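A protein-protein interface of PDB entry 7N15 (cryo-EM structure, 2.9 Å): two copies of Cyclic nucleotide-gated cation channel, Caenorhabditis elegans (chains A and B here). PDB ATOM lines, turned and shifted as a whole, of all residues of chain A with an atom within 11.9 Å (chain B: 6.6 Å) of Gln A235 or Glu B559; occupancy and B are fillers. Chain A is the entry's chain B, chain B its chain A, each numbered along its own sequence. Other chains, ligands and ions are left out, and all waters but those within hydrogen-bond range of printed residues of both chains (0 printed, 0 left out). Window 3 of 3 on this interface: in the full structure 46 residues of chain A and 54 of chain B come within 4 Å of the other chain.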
ATOM      1  N   ASP A 120      24.008   2.208  13.739  1.00  0.00           N
ATOM      2  CA  ASP A 120      23.080   1.945  12.650  1.00  0.00           C
ATOM      3  C   ASP A 120      23.485   2.799  11.461  1.00  0.00           C
ATOM      4  O   ASP A 120      23.494   4.033  11.583  1.00  0.00           O
ATOM      5  CB  ASP A 120      21.656   2.276  13.083  1.00  0.00           C
ATOM      6  CG  ASP A 120      20.596   1.577  12.250  1.00  0.00           C
ATOM      7  OD1 ASP A 120      20.878   1.152  11.115  1.00  0.00           O
ATOM      8  OD2 ASP A 120      19.454   1.461  12.738  1.00  0.00           O
ATOM      9  N   PRO A 121      23.831   2.216  10.313  1.00  0.00           N
ATOM     10  CA  PRO A 121      24.281   3.045   9.184  1.00  0.00           C
ATOM     11  C   PRO A 121      23.159   3.767   8.459  1.00  0.00           C
ATOM     12  O   PRO A 121      23.436   4.653   7.639  1.00  0.00           O
ATOM     13  CB  PRO A 121      24.975   2.030   8.269  1.00  0.00           C
ATOM     14  CG  PRO A 121      24.341   0.742   8.594  1.00  0.00           C
ATOM     15  CD  PRO A 121      24.026   0.781  10.052  1.00  0.00           C
ATOM     16  N   GLY A 231      26.782  -1.595  12.310  1.00  0.00           N
ATOM     17  CA  GLY A 231      25.749  -2.557  12.008  1.00  0.00           C
ATOM     18  C   GLY A 231      25.646  -2.826  10.526  1.00  0.00           C
ATOM     19  O   GLY A 231      25.986  -1.999   9.685  1.00  0.00           O
ATOM     20  N   TYR A 232      25.159  -4.018  10.204  1.00  0.00           N
ATOM     21  CA  TYR A 232      25.131  -4.477   8.828  1.00  0.00           C
ATOM     22  C   TYR A 232      23.820  -5.201   8.581  1.00  0.00           C
ATOM     23  O   TYR A 232      23.264  -5.825   9.487  1.00  0.00           O
ATOM     24  CB  TYR A 232      26.331  -5.384   8.510  1.00  0.00           C
ATOM     25  CG  TYR A 232      26.367  -6.710   9.248  1.00  0.00           C
ATOM     26  CD1 TYR A 232      26.824  -6.790  10.559  1.00  0.00           C
ATOM     27  CD2 TYR A 232      25.978  -7.886   8.618  1.00  0.00           C
ATOM     28  CE1 TYR A 232      26.862  -7.995  11.230  1.00  0.00           C
ATOM     29  CE2 TYR A 232      26.016  -9.097   9.281  1.00  0.00           C
ATOM     30  CZ  TYR A 232      26.460  -9.143  10.585  1.00  0.00           C
ATOM     31  OH  TYR A 232      26.500 -10.347  11.244  1.00  0.00           O
ATOM     32  N   MET A 233      23.327  -5.099   7.350  1.00  0.00           N
ATOM     33  CA  MET A 233      22.080  -5.751   6.984  1.00  0.00           C
ATOM     34  C   MET A 233      22.267  -7.258   6.889  1.00  0.00           C
ATOM     35  O   MET A 233      23.189  -7.747   6.232  1.00  0.00           O
ATOM     36  CB  MET A 233      21.566  -5.210   5.653  1.00  0.00           C
ATOM     37  CG  MET A 233      21.671  -3.709   5.508  1.00  0.00           C
ATOM     38  SD  MET A 233      20.402  -2.836   6.432  1.00  0.00           S
ATOM     39  CE  MET A 233      18.947  -3.293   5.509  1.00  0.00           C
ATOM     40  N   ASP A 234      21.378  -7.999   7.552  1.00  0.00           N
ATOM     41  CA  ASP A 234      21.415  -9.458   7.518  1.00  0.00           C
ATOM     42  C   ASP A 234      20.251  -9.996   6.704  1.00  0.00           C
ATOM     43  O   ASP A 234      20.466 -10.716   5.727  1.00  0.00           O
ATOM     44  CB  ASP A 234      21.396 -10.006   8.947  1.00  0.00           C
ATOM     45  CG  ASP A 234      22.007 -11.389   9.057  1.00  0.00           C
ATOM     46  OD1 ASP A 234      22.270 -12.022   8.012  1.00  0.00           O
ATOM     47  OD2 ASP A 234      22.223 -11.848  10.198  1.00  0.00           O
ATOM     48  N   GLN A 235      19.017  -9.658   7.067  1.00  0.00           N
ATOM     49  CA  GLN A 235      17.820 -10.069   6.347  1.00  0.00           C
ATOM     50  C   GLN A 235      16.914  -8.852   6.202  1.00  0.00           C
ATOM     51  O   GLN A 235      15.742  -8.862   6.573  1.00  0.00           O
ATOM     52  CB  GLN A 235      17.115 -11.220   7.056  1.00  0.00           C
ATOM     53  CG  GLN A 235      17.796 -12.569   6.878  1.00  0.00           C
ATOM     54  CD  GLN A 235      17.713 -13.094   5.455  1.00  0.00           C
ATOM     55  OE1 GLN A 235      18.672 -13.006   4.691  1.00  0.00           O
ATOM     56  NE2 GLN A 235      16.565 -13.653   5.099  1.00  0.00           N
ATOM     57  N   GLY A 236      17.497  -7.756   5.727  1.00  0.00           N
ATOM     58  CA  GLY A 236      16.799  -6.494   5.670  1.00  0.00           C
ATOM     59  C   GLY A 236      16.768  -5.729   6.973  1.00  0.00           C
ATOM     60  O   GLY A 236      16.172  -4.646   7.022  1.00  0.00           O
ATOM     61  N   LEU A 237      17.387  -6.252   8.024  1.00  0.00           N
ATOM     62  CA  LEU A 237      17.475  -5.591   9.314  1.00  0.00           C
ATOM     63  C   LEU A 237      18.936  -5.500   9.714  1.00  0.00           C
ATOM     64  O   LEU A 237      19.734  -6.372   9.366  1.00  0.00           O
ATOM     65  CB  LEU A 237      16.697  -6.349  10.387  1.00  0.00           C
ATOM     66  CG  LEU A 237      15.183  -6.430  10.238  1.00  0.00           C
ATOM     67  CD1 LEU A 237      14.773  -7.796   9.721  1.00  0.00           C
ATOM     68  CD2 LEU A 237      14.529  -6.136  11.569  1.00  0.00           C
ATOM     69  N   VAL A 238      19.282  -4.446  10.437  1.00  0.00           N
ATOM     70  CA  VAL A 238      20.650  -4.276  10.910  1.00  0.00           C
ATOM     71  C   VAL A 238      20.888  -5.178  12.114  1.00  0.00           C
ATOM     72  O   VAL A 238      20.004  -5.375  12.954  1.00  0.00           O
ATOM     73  CB  VAL A 238      20.937  -2.799  11.240  1.00  0.00           C
ATOM     74  CG1 VAL A 238      21.110  -2.002   9.970  1.00  0.00           C
ATOM     75  CG2 VAL A 238      19.818  -2.202  12.064  1.00  0.00           C
ATOM     76  N   VAL A 239      22.083  -5.761  12.176  1.00  0.00           N
ATOM     77  CA  VAL A 239      22.507  -6.459  13.379  1.00  0.00           C
ATOM     78  C   VAL A 239      23.088  -5.444  14.347  1.00  0.00           C
ATOM     79  O   VAL A 239      23.956  -4.642  13.982  1.00  0.00           O
ATOM     80  CB  VAL A 239      23.533  -7.551  13.037  1.00  0.00           C
ATOM     81  CG1 VAL A 239      23.718  -8.483  14.209  1.00  0.00           C
ATOM     82  CG2 VAL A 239      23.088  -8.314  11.817  1.00  0.00           C
ATOM     83  N   ARG A 240      22.597  -5.442  15.580  1.00  0.00           N
ATOM     84  CA  ARG A 240      22.982  -4.392  16.511  1.00  0.00           C
ATOM     85  C   ARG A 240      23.324  -4.949  17.884  1.00  0.00           C
ATOM     86  O   ARG A 240      22.931  -4.394  18.914  1.00  0.00           O
ATOM     87  CB  ARG A 240      21.899  -3.321  16.601  1.00  0.00           C
ATOM     88  CG  ARG A 240      21.997  -2.276  15.494  1.00  0.00           C
ATOM     89  CD  ARG A 240      21.303  -0.989  15.863  1.00  0.00           C
ATOM     90  NE  ARG A 240      22.005  -0.299  16.933  1.00  0.00           N
ATOM     91  CZ  ARG A 240      21.567   0.806  17.522  1.00  0.00           C
ATOM     92  NH1 ARG A 240      20.425   1.353  17.139  1.00  0.00           N
ATOM     93  NH2 ARG A 240      22.272   1.366  18.493  1.00  0.00           N
ATOM     94  N   GLU A 241      24.072  -6.049  17.924  1.00  0.00           N
ATOM     95  CA  GLU A 241      24.799  -6.418  19.129  1.00  0.00           C
ATOM     96  C   GLU A 241      26.266  -6.559  18.761  1.00  0.00           C
ATOM     97  O   GLU A 241      26.606  -6.854  17.614  1.00  0.00           O
ATOM     98  CB  GLU A 241      24.261  -7.695  19.794  1.00  0.00           C
ATOM     99  CG  GLU A 241      24.386  -8.966  18.983  1.00  0.00           C
ATOM    100  CD  GLU A 241      23.117  -9.293  18.224  1.00  0.00           C
ATOM    101  OE1 GLU A 241      22.237  -8.415  18.117  1.00  0.00           O
ATOM    102  OE2 GLU A 241      22.993 -10.437  17.742  1.00  0.00           O
ATOM    103  N   LYS A 244      28.649  -9.731  16.824  1.00  0.00           N
ATOM    104  CA  LYS A 244      28.489 -10.016  15.403  1.00  0.00           C
ATOM    105  C   LYS A 244      29.046  -8.892  14.538  1.00  0.00           C
ATOM    106  O   LYS A 244      29.683  -9.159  13.513  1.00  0.00           O
ATOM    107  CB  LYS A 244      27.015 -10.261  15.083  1.00  0.00           C
ATOM    108  CG  LYS A 244      26.404 -11.411  15.865  1.00  0.00           C
ATOM    109  CD  LYS A 244      25.073 -11.838  15.280  1.00  0.00           C
ATOM    110  CE  LYS A 244      25.237 -12.377  13.870  1.00  0.00           C
ATOM    111  NZ  LYS A 244      23.926 -12.696  13.244  1.00  0.00           N
ATOM    112  N   VAL A 245      28.872  -7.639  14.961  1.00  0.00           N
ATOM    113  CA  VAL A 245      29.382  -6.533  14.158  1.00  0.00           C
ATOM    114  C   VAL A 245      30.895  -6.402  14.293  1.00  0.00           C
ATOM    115  O   VAL A 245      31.567  -6.022  13.328  1.00  0.00           O
ATOM    116  CB  VAL A 245      28.654  -5.218  14.492  1.00  0.00           C
ATOM    117  CG1 VAL A 245      27.206  -5.328  14.111  1.00  0.00           C
ATOM    118  CG2 VAL A 245      28.769  -4.856  15.950  1.00  0.00           C
ATOM    119  N   TYR B 459      17.989   2.149  -0.226  1.00  0.00           N
ATOM    120  CA  TYR B 459      18.199   0.710  -0.110  1.00  0.00           C
ATOM    121  C   TYR B 459      18.515   0.080  -1.460  1.00  0.00           C
ATOM    122  O   TYR B 459      19.299  -0.871  -1.530  1.00  0.00           O
ATOM    123  CB  TYR B 459      16.981   0.034   0.509  1.00  0.00           C
ATOM    124  CG  TYR B 459      17.161  -1.457   0.718  1.00  0.00           C
ATOM    125  CD1 TYR B 459      16.588  -2.377  -0.154  1.00  0.00           C
ATOM    126  CD2 TYR B 459      17.901  -1.942   1.786  1.00  0.00           C
ATOM    127  CE1 TYR B 459      16.754  -3.732   0.027  1.00  0.00           C
ATOM    128  CE2 TYR B 459      18.068  -3.300   1.976  1.00  0.00           C
ATOM    129  CZ  TYR B 459      17.494  -4.187   1.091  1.00  0.00           C
ATOM    130  OH  TYR B 459      17.649  -5.540   1.277  1.00  0.00           O
ATOM    131  N   GLU B 491      21.262 -20.869  -3.795  1.00  0.00           N
ATOM    132  CA  GLU B 491      21.055 -21.015  -2.359  1.00  0.00           C
ATOM    133  C   GLU B 491      19.654 -20.604  -1.933  1.00  0.00           C
ATOM    134  O   GLU B 491      19.165 -21.087  -0.909  1.00  0.00           O
ATOM    135  CB  GLU B 491      22.089 -20.192  -1.590  1.00  0.00           C
ATOM    136  CG  GLU B 491      23.535 -20.687  -1.679  1.00  0.00           C
ATOM    137  CD  GLU B 491      23.679 -22.200  -1.604  1.00  0.00           C
ATOM    138  OE1 GLU B 491      24.298 -22.777  -2.522  1.00  0.00           O
ATOM    139  OE2 GLU B 491      23.221 -22.809  -0.612  1.00  0.00           O
ATOM    140  N   THR B 492      18.999 -19.731  -2.698  1.00  0.00           N
ATOM    141  CA  THR B 492      17.623 -19.360  -2.387  1.00  0.00           C
ATOM    142  C   THR B 492      16.648 -20.419  -2.882  1.00  0.00           C
ATOM    143  O   THR B 492      15.765 -20.854  -2.136  1.00  0.00           O
ATOM    144  CB  THR B 492      17.301 -18.000  -3.001  1.00  0.00           C
ATOM    145  OG1 THR B 492      18.195 -17.016  -2.473  1.00  0.00           O
ATOM    146  CG2 THR B 492      15.876 -17.592  -2.688  1.00  0.00           C
ATOM    147  N   LYS B 495      16.118 -23.821  -1.071  1.00  0.00           N
ATOM    148  CA  LYS B 495      15.252 -23.841   0.100  1.00  0.00           C
ATOM    149  C   LYS B 495      13.773 -23.922  -0.249  1.00  0.00           C
ATOM    150  O   LYS B 495      12.944 -24.003   0.663  1.00  0.00           O
ATOM    151  CB  LYS B 495      15.490 -22.595   0.954  1.00  0.00           C
ATOM    152  CG  LYS B 495      16.930 -22.368   1.350  1.00  0.00           C
ATOM    153  CD  LYS B 495      17.022 -21.319   2.441  1.00  0.00           C
ATOM    154  CE  LYS B 495      18.455 -21.074   2.861  1.00  0.00           C
ATOM    155  NZ  LYS B 495      19.249 -20.463   1.768  1.00  0.00           N
ATOM    156  N   VAL B 538      10.473 -15.850  -1.057  1.00  0.00           N
ATOM    157  CA  VAL B 538      11.320 -14.889  -0.358  1.00  0.00           C
ATOM    158  C   VAL B 538      12.762 -15.062  -0.819  1.00  0.00           C
ATOM    159  O   VAL B 538      13.383 -16.100  -0.572  1.00  0.00           O
ATOM    160  CB  VAL B 538      11.204 -15.062   1.159  1.00  0.00           C
ATOM    161  CG1 VAL B 538      11.992 -13.999   1.874  1.00  0.00           C
ATOM    162  CG2 VAL B 538       9.765 -15.047   1.586  1.00  0.00           C
ATOM    163  N   LYS B 539      13.297 -14.044  -1.489  1.00  0.00           N
ATOM    164  CA  LYS B 539      14.706 -14.038  -1.859  1.00  0.00           C
ATOM    165  C   LYS B 539      15.577 -13.564  -0.708  1.00  0.00           C
ATOM    166  O   LYS B 539      16.578 -14.205  -0.379  1.00  0.00           O
ATOM    167  CB  LYS B 539      14.919 -13.152  -3.089  1.00  0.00           C
ATOM    168  CG  LYS B 539      16.366 -12.798  -3.389  1.00  0.00           C
ATOM    169  CD  LYS B 539      17.159 -14.008  -3.849  1.00  0.00           C
ATOM    170  CE  LYS B 539      18.632 -13.687  -3.989  1.00  0.00           C
ATOM    171  NZ  LYS B 539      19.453 -14.918  -4.114  1.00  0.00           N
ATOM    172  N   ARG B 540      15.208 -12.451  -0.087  1.00  0.00           N
ATOM    173  CA  ARG B 540      15.878 -11.958   1.103  1.00  0.00           C
ATOM    174  C   ARG B 540      14.811 -11.401   2.023  1.00  0.00           C
ATOM    175  O   ARG B 540      13.697 -11.100   1.592  1.00  0.00           O
ATOM    176  CB  ARG B 540      16.906 -10.874   0.776  1.00  0.00           C
ATOM    177  CG  ARG B 540      18.271 -11.388   0.388  1.00  0.00           C
ATOM    178  CD  ARG B 540      19.169 -10.234   0.008  1.00  0.00           C
ATOM    179  NE  ARG B 540      19.281  -9.277   1.100  1.00  0.00           N
ATOM    180  CZ  ARG B 540      19.892  -8.103   1.003  1.00  0.00           C
ATOM    181  NH1 ARG B 540      19.946  -7.296   2.054  1.00  0.00           N
ATOM    182  NH2 ARG B 540      20.442  -7.734  -0.145  1.00  0.00           N
ATOM    183  N   GLY B 541      15.154 -11.267   3.289  1.00  0.00           N
ATOM    184  CA  GLY B 541      14.276 -10.581   4.207  1.00  0.00           C
ATOM    185  C   GLY B 541      13.510 -11.516   5.122  1.00  0.00           C
ATOM    186  O   GLY B 541      13.535 -12.737   4.987  1.00  0.00           O
ATOM    187  N   ARG B 542      12.831 -10.908   6.087  1.00  0.00           N
ATOM    188  CA  ARG B 542      11.996 -11.609   7.046  1.00  0.00           C
ATOM    189  C   ARG B 542      10.607 -10.990   7.043  1.00  0.00           C
ATOM    190  O   ARG B 542      10.466  -9.767   6.956  1.00  0.00           O
ATOM    191  CB  ARG B 542      12.602 -11.536   8.448  1.00  0.00           C
ATOM    192  CG  ARG B 542      12.238 -12.689   9.352  1.00  0.00           C
ATOM    193  CD  ARG B 542      12.956 -12.572  10.684  1.00  0.00           C
ATOM    194  NE  ARG B 542      12.475 -11.428  11.453  1.00  0.00           N
ATOM    195  CZ  ARG B 542      13.028 -10.998  12.581  1.00  0.00           C
ATOM    196  NH1 ARG B 542      12.519  -9.950  13.214  1.00  0.00           N
ATOM    197  NH2 ARG B 542      14.091 -11.614  13.076  1.00  0.00           N
ATOM    198  N   LEU B 557       8.229 -15.672   8.286  1.00  0.00           N
ATOM    199  CA  LEU B 557       8.634 -16.187   6.987  1.00  0.00           C
ATOM    200  C   LEU B 557      10.058 -15.741   6.704  1.00  0.00           C
ATOM    201  O   LEU B 557      10.359 -14.545   6.745  1.00  0.00           O
ATOM    202  CB  LEU B 557       7.681 -15.709   5.889  1.00  0.00           C
ATOM    203  CG  LEU B 557       6.240 -16.206   6.016  1.00  0.00           C
ATOM    204  CD1 LEU B 557       5.361 -15.545   4.987  1.00  0.00           C
ATOM    205  CD2 LEU B 557       6.186 -17.709   5.870  1.00  0.00           C
ATOM    206  N   GLN B 558      10.930 -16.704   6.423  1.00  0.00           N
ATOM    207  CA  GLN B 558      12.347 -16.483   6.218  1.00  0.00           C
ATOM    208  C   GLN B 558      12.668 -16.688   4.738  1.00  0.00           C
ATOM    209  O   GLN B 558      11.756 -16.827   3.917  1.00  0.00           O
ATOM    210  CB  GLN B 558      13.142 -17.409   7.139  1.00  0.00           C
ATOM    211  CG  GLN B 558      12.620 -17.459   8.561  1.00  0.00           C
ATOM    212  CD  GLN B 558      13.299 -16.452   9.468  1.00  0.00           C
ATOM    213  OE1 GLN B 558      14.392 -15.970   9.172  1.00  0.00           O
ATOM    214  NE2 GLN B 558      12.648 -16.123  10.577  1.00  0.00           N
ATOM    215  N   GLU B 559      13.956 -16.673   4.401  1.00  0.00           N
ATOM    216  CA  GLU B 559      14.403 -16.850   3.024  1.00  0.00           C
ATOM    217  C   GLU B 559      14.074 -18.249   2.508  1.00  0.00           C
ATOM    218  O   GLU B 559      14.375 -19.254   3.155  1.00  0.00           O
ATOM    219  CB  GLU B 559      15.909 -16.608   2.927  1.00  0.00           C
ATOM    220  CG  GLU B 559      16.499 -16.881   1.559  1.00  0.00           C
ATOM    221  CD  GLU B 559      18.000 -17.079   1.590  1.00  0.00           C
ATOM    222  OE1 GLU B 559      18.507 -17.665   2.568  1.00  0.00           O
ATOM    223  OE2 GLU B 559      18.675 -16.647   0.634  1.00  0.00           O
ATOM    224  N   GLY B 560      13.444 -18.302   1.337  1.00  0.00           N
ATOM    225  CA  GLY B 560      13.009 -19.545   0.748  1.00  0.00           C
ATOM    226  C   GLY B 560      11.583 -19.933   1.060  1.00  0.00           C
ATOM    227  O   GLY B 560      11.120 -20.967   0.565  1.00  0.00           O
ATOM    228  N   SER B 561      10.874 -19.144   1.860  1.00  0.00           N
ATOM    229  CA  SER B 561       9.491 -19.454   2.179  1.00  0.00           C
ATOM    230  C   SER B 561       8.582 -19.119   1.004  1.00  0.00           C
ATOM    231  O   SER B 561       8.838 -18.194   0.234  1.00  0.00           O
ATOM    232  CB  SER B 561       9.040 -18.687   3.416  1.00  0.00           C
ATOM    233  OG  SER B 561       9.764 -19.108   4.556  1.00  0.00           O
ATOM    234  N   VAL B 587       9.139  -7.242   7.857  1.00  0.00           N
ATOM    235  CA  VAL B 587       9.786  -6.796   9.085  1.00  0.00           C
ATOM    236  C   VAL B 587      10.822  -5.742   8.725  1.00  0.00           C
ATOM    237  O   VAL B 587      10.749  -4.599   9.187  1.00  0.00           O
ATOM    238  CB  VAL B 587      10.429  -7.969   9.842  1.00  0.00           C
ATOM    239  CG1 VAL B 587      11.021  -7.491  11.142  1.00  0.00           C
ATOM    240  CG2 VAL B 587       9.411  -9.047  10.101  1.00  0.00           C
ATOM    241  N   GLY B 588      11.789  -6.120   7.900  1.00  0.00           N
ATOM    242  CA  GLY B 588      12.727  -5.192   7.319  1.00  0.00           C
ATOM    243  C   GLY B 588      12.480  -5.010   5.839  1.00  0.00           C
ATOM    244  O   GLY B 588      11.358  -5.157   5.346  1.00  0.00           O
ATOM    245  N   TYR B 589      13.542  -4.683   5.116  1.00  0.00           N
ATOM    246  CA  TYR B 589      13.452  -4.662   3.667  1.00  0.00           C
ATOM    247  C   TYR B 589      13.447  -6.088   3.136  1.00  0.00           C
ATOM    248  O   TYR B 589      14.196  -6.944   3.610  1.00  0.00           O
ATOM    249  CB  TYR B 589      14.612  -3.882   3.072  1.00  0.00           C
ATOM    250  CG  TYR B 589      14.501  -2.388   3.207  1.00  0.00           C
ATOM    251  CD1 TYR B 589      13.842  -1.635   2.245  1.00  0.00           C
ATOM    252  CD2 TYR B 589      15.074  -1.726   4.283  1.00  0.00           C
ATOM    253  CE1 TYR B 589      13.747  -0.267   2.356  1.00  0.00           C
ATOM    254  CE2 TYR B 589      14.987  -0.358   4.402  1.00  0.00           C
ATOM    255  CZ  TYR B 589      14.320   0.362   3.438  1.00  0.00           C
ATOM    256  OH  TYR B 589      14.226   1.724   3.558  1.00  0.00           O
ATOM    257  N   THR B 590      12.599  -6.348   2.147  1.00  0.00           N
ATOM    258  CA  THR B 590      12.321  -7.716   1.726  1.00  0.00           C
ATOM    259  C   THR B 590      12.344  -7.794   0.208  1.00  0.00           C
ATOM    260  O   THR B 590      11.567  -7.109  -0.458  1.00  0.00           O
ATOM    261  CB  THR B 590      10.973  -8.185   2.264  1.00  0.00           C
ATOM    262  OG1 THR B 590      10.986  -8.138   3.692  1.00  0.00           O
ATOM    263  CG2 THR B 590      10.701  -9.595   1.832  1.00  0.00           C
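Met A233 touches Tyr B459 (CE to CE2, 3.6 Å).
Arg B542 touches Gln A235.
NE2 of Gln A235 touches CB of Glu B559, 3.7 Å away.
Tyr B589 touches Gln A235.
Gly A236 touches Gly B588 (O to CA, 3.5 Å).
CD2 of Leu A237 touches CG1 of Val B587, 3.8 Å away.
Gly B588 touches Leu A237 (N to CD1, 3.9 Å).
N of Tyr B589 is in hydrogen-bond range of O of Gly A236 (3.2 Å).
The backbone carbonyl oxygen (O) of Gly B541 is in hydrogen-bond range of the side-chain amide nitrogen (NE2) of Gln A235.
NZ of Lys B495 lies within salt-bridge range of OE1 of Glu B559, at 3.0 Å.
The backbone NH (N) of Val B587 lies within hydrogen-bond range of the backbone carbonyl oxygen (O) of Arg B542.
The side-chain hydroxyl (OG1) of Thr B590 lies within hydrogen-bond range of the backbone carbonyl oxygen (O) of Gly B588 (3.4 Å).
The guanidinium group of Arg B540 is in hydrogen-bond range of the side-chain hydroxyl of Tyr B459, 3.0 Å away.
The side-chain carboxylate of Glu B559 is in hydrogen-bond range of the side-chain hydroxyl of Thr B492 (3.2 Å).
Of the 15 printed residues of chain A, 4 touch a printed residue of chain B.
Printed residues of chain B that touch a printed residue of chain A: Tyr B459, Gly B541, Arg B542, Glu B559, Val B587, Gly B588 and Tyr B589.
Hydrophobic or aromatic side chains of chain B within 4 Å of the printed part of chain A: Tyr B459 and Val B587.
Of the printed residues of chain B, Gly A236 touches Gly B588 and Tyr B589.
Of the printed residues of chain B, Leu A237 touches Val B587 (3.8 Å) and Gly B588 (3.9 Å).
Of the printed residues of chain A, Tyr B459 touches Met A233 (3.6 Å).
No residue of chain A comes within 4 Å of Thr B492.
No residue of chain A comes within 4 Å of Lys B495.
No residue of chain A comes within 4 Å of Lys B539.
No residue of chain A comes within 4 Å of Arg B540.
Gly B541 touches just one residue of chain A: Gln A235 (3.2 Å).
Of chain A, only Gln A235 comes within 4 Å of Arg B542.
Gln B558 touches none of the printed residues of chain A.
Of chain A, only Gln A235 (3.7 Å) comes within 4 Å of Glu B559.
Gly B560 touches none of the printed residues of chain A.
No residue of chain A comes within 4 Å of Ser B561.
Of chain A, only Gly A236 and Leu A237 come within 4 Å of Gly B588.
The nearest residue of chain A that does not touch Glu B559 is Asp A234 (7.9 Å).
No position is printed for both chains.
Of the 9 pairs that touch across the chains among the printed residues, none has its exchanged pair printed and touching as well.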
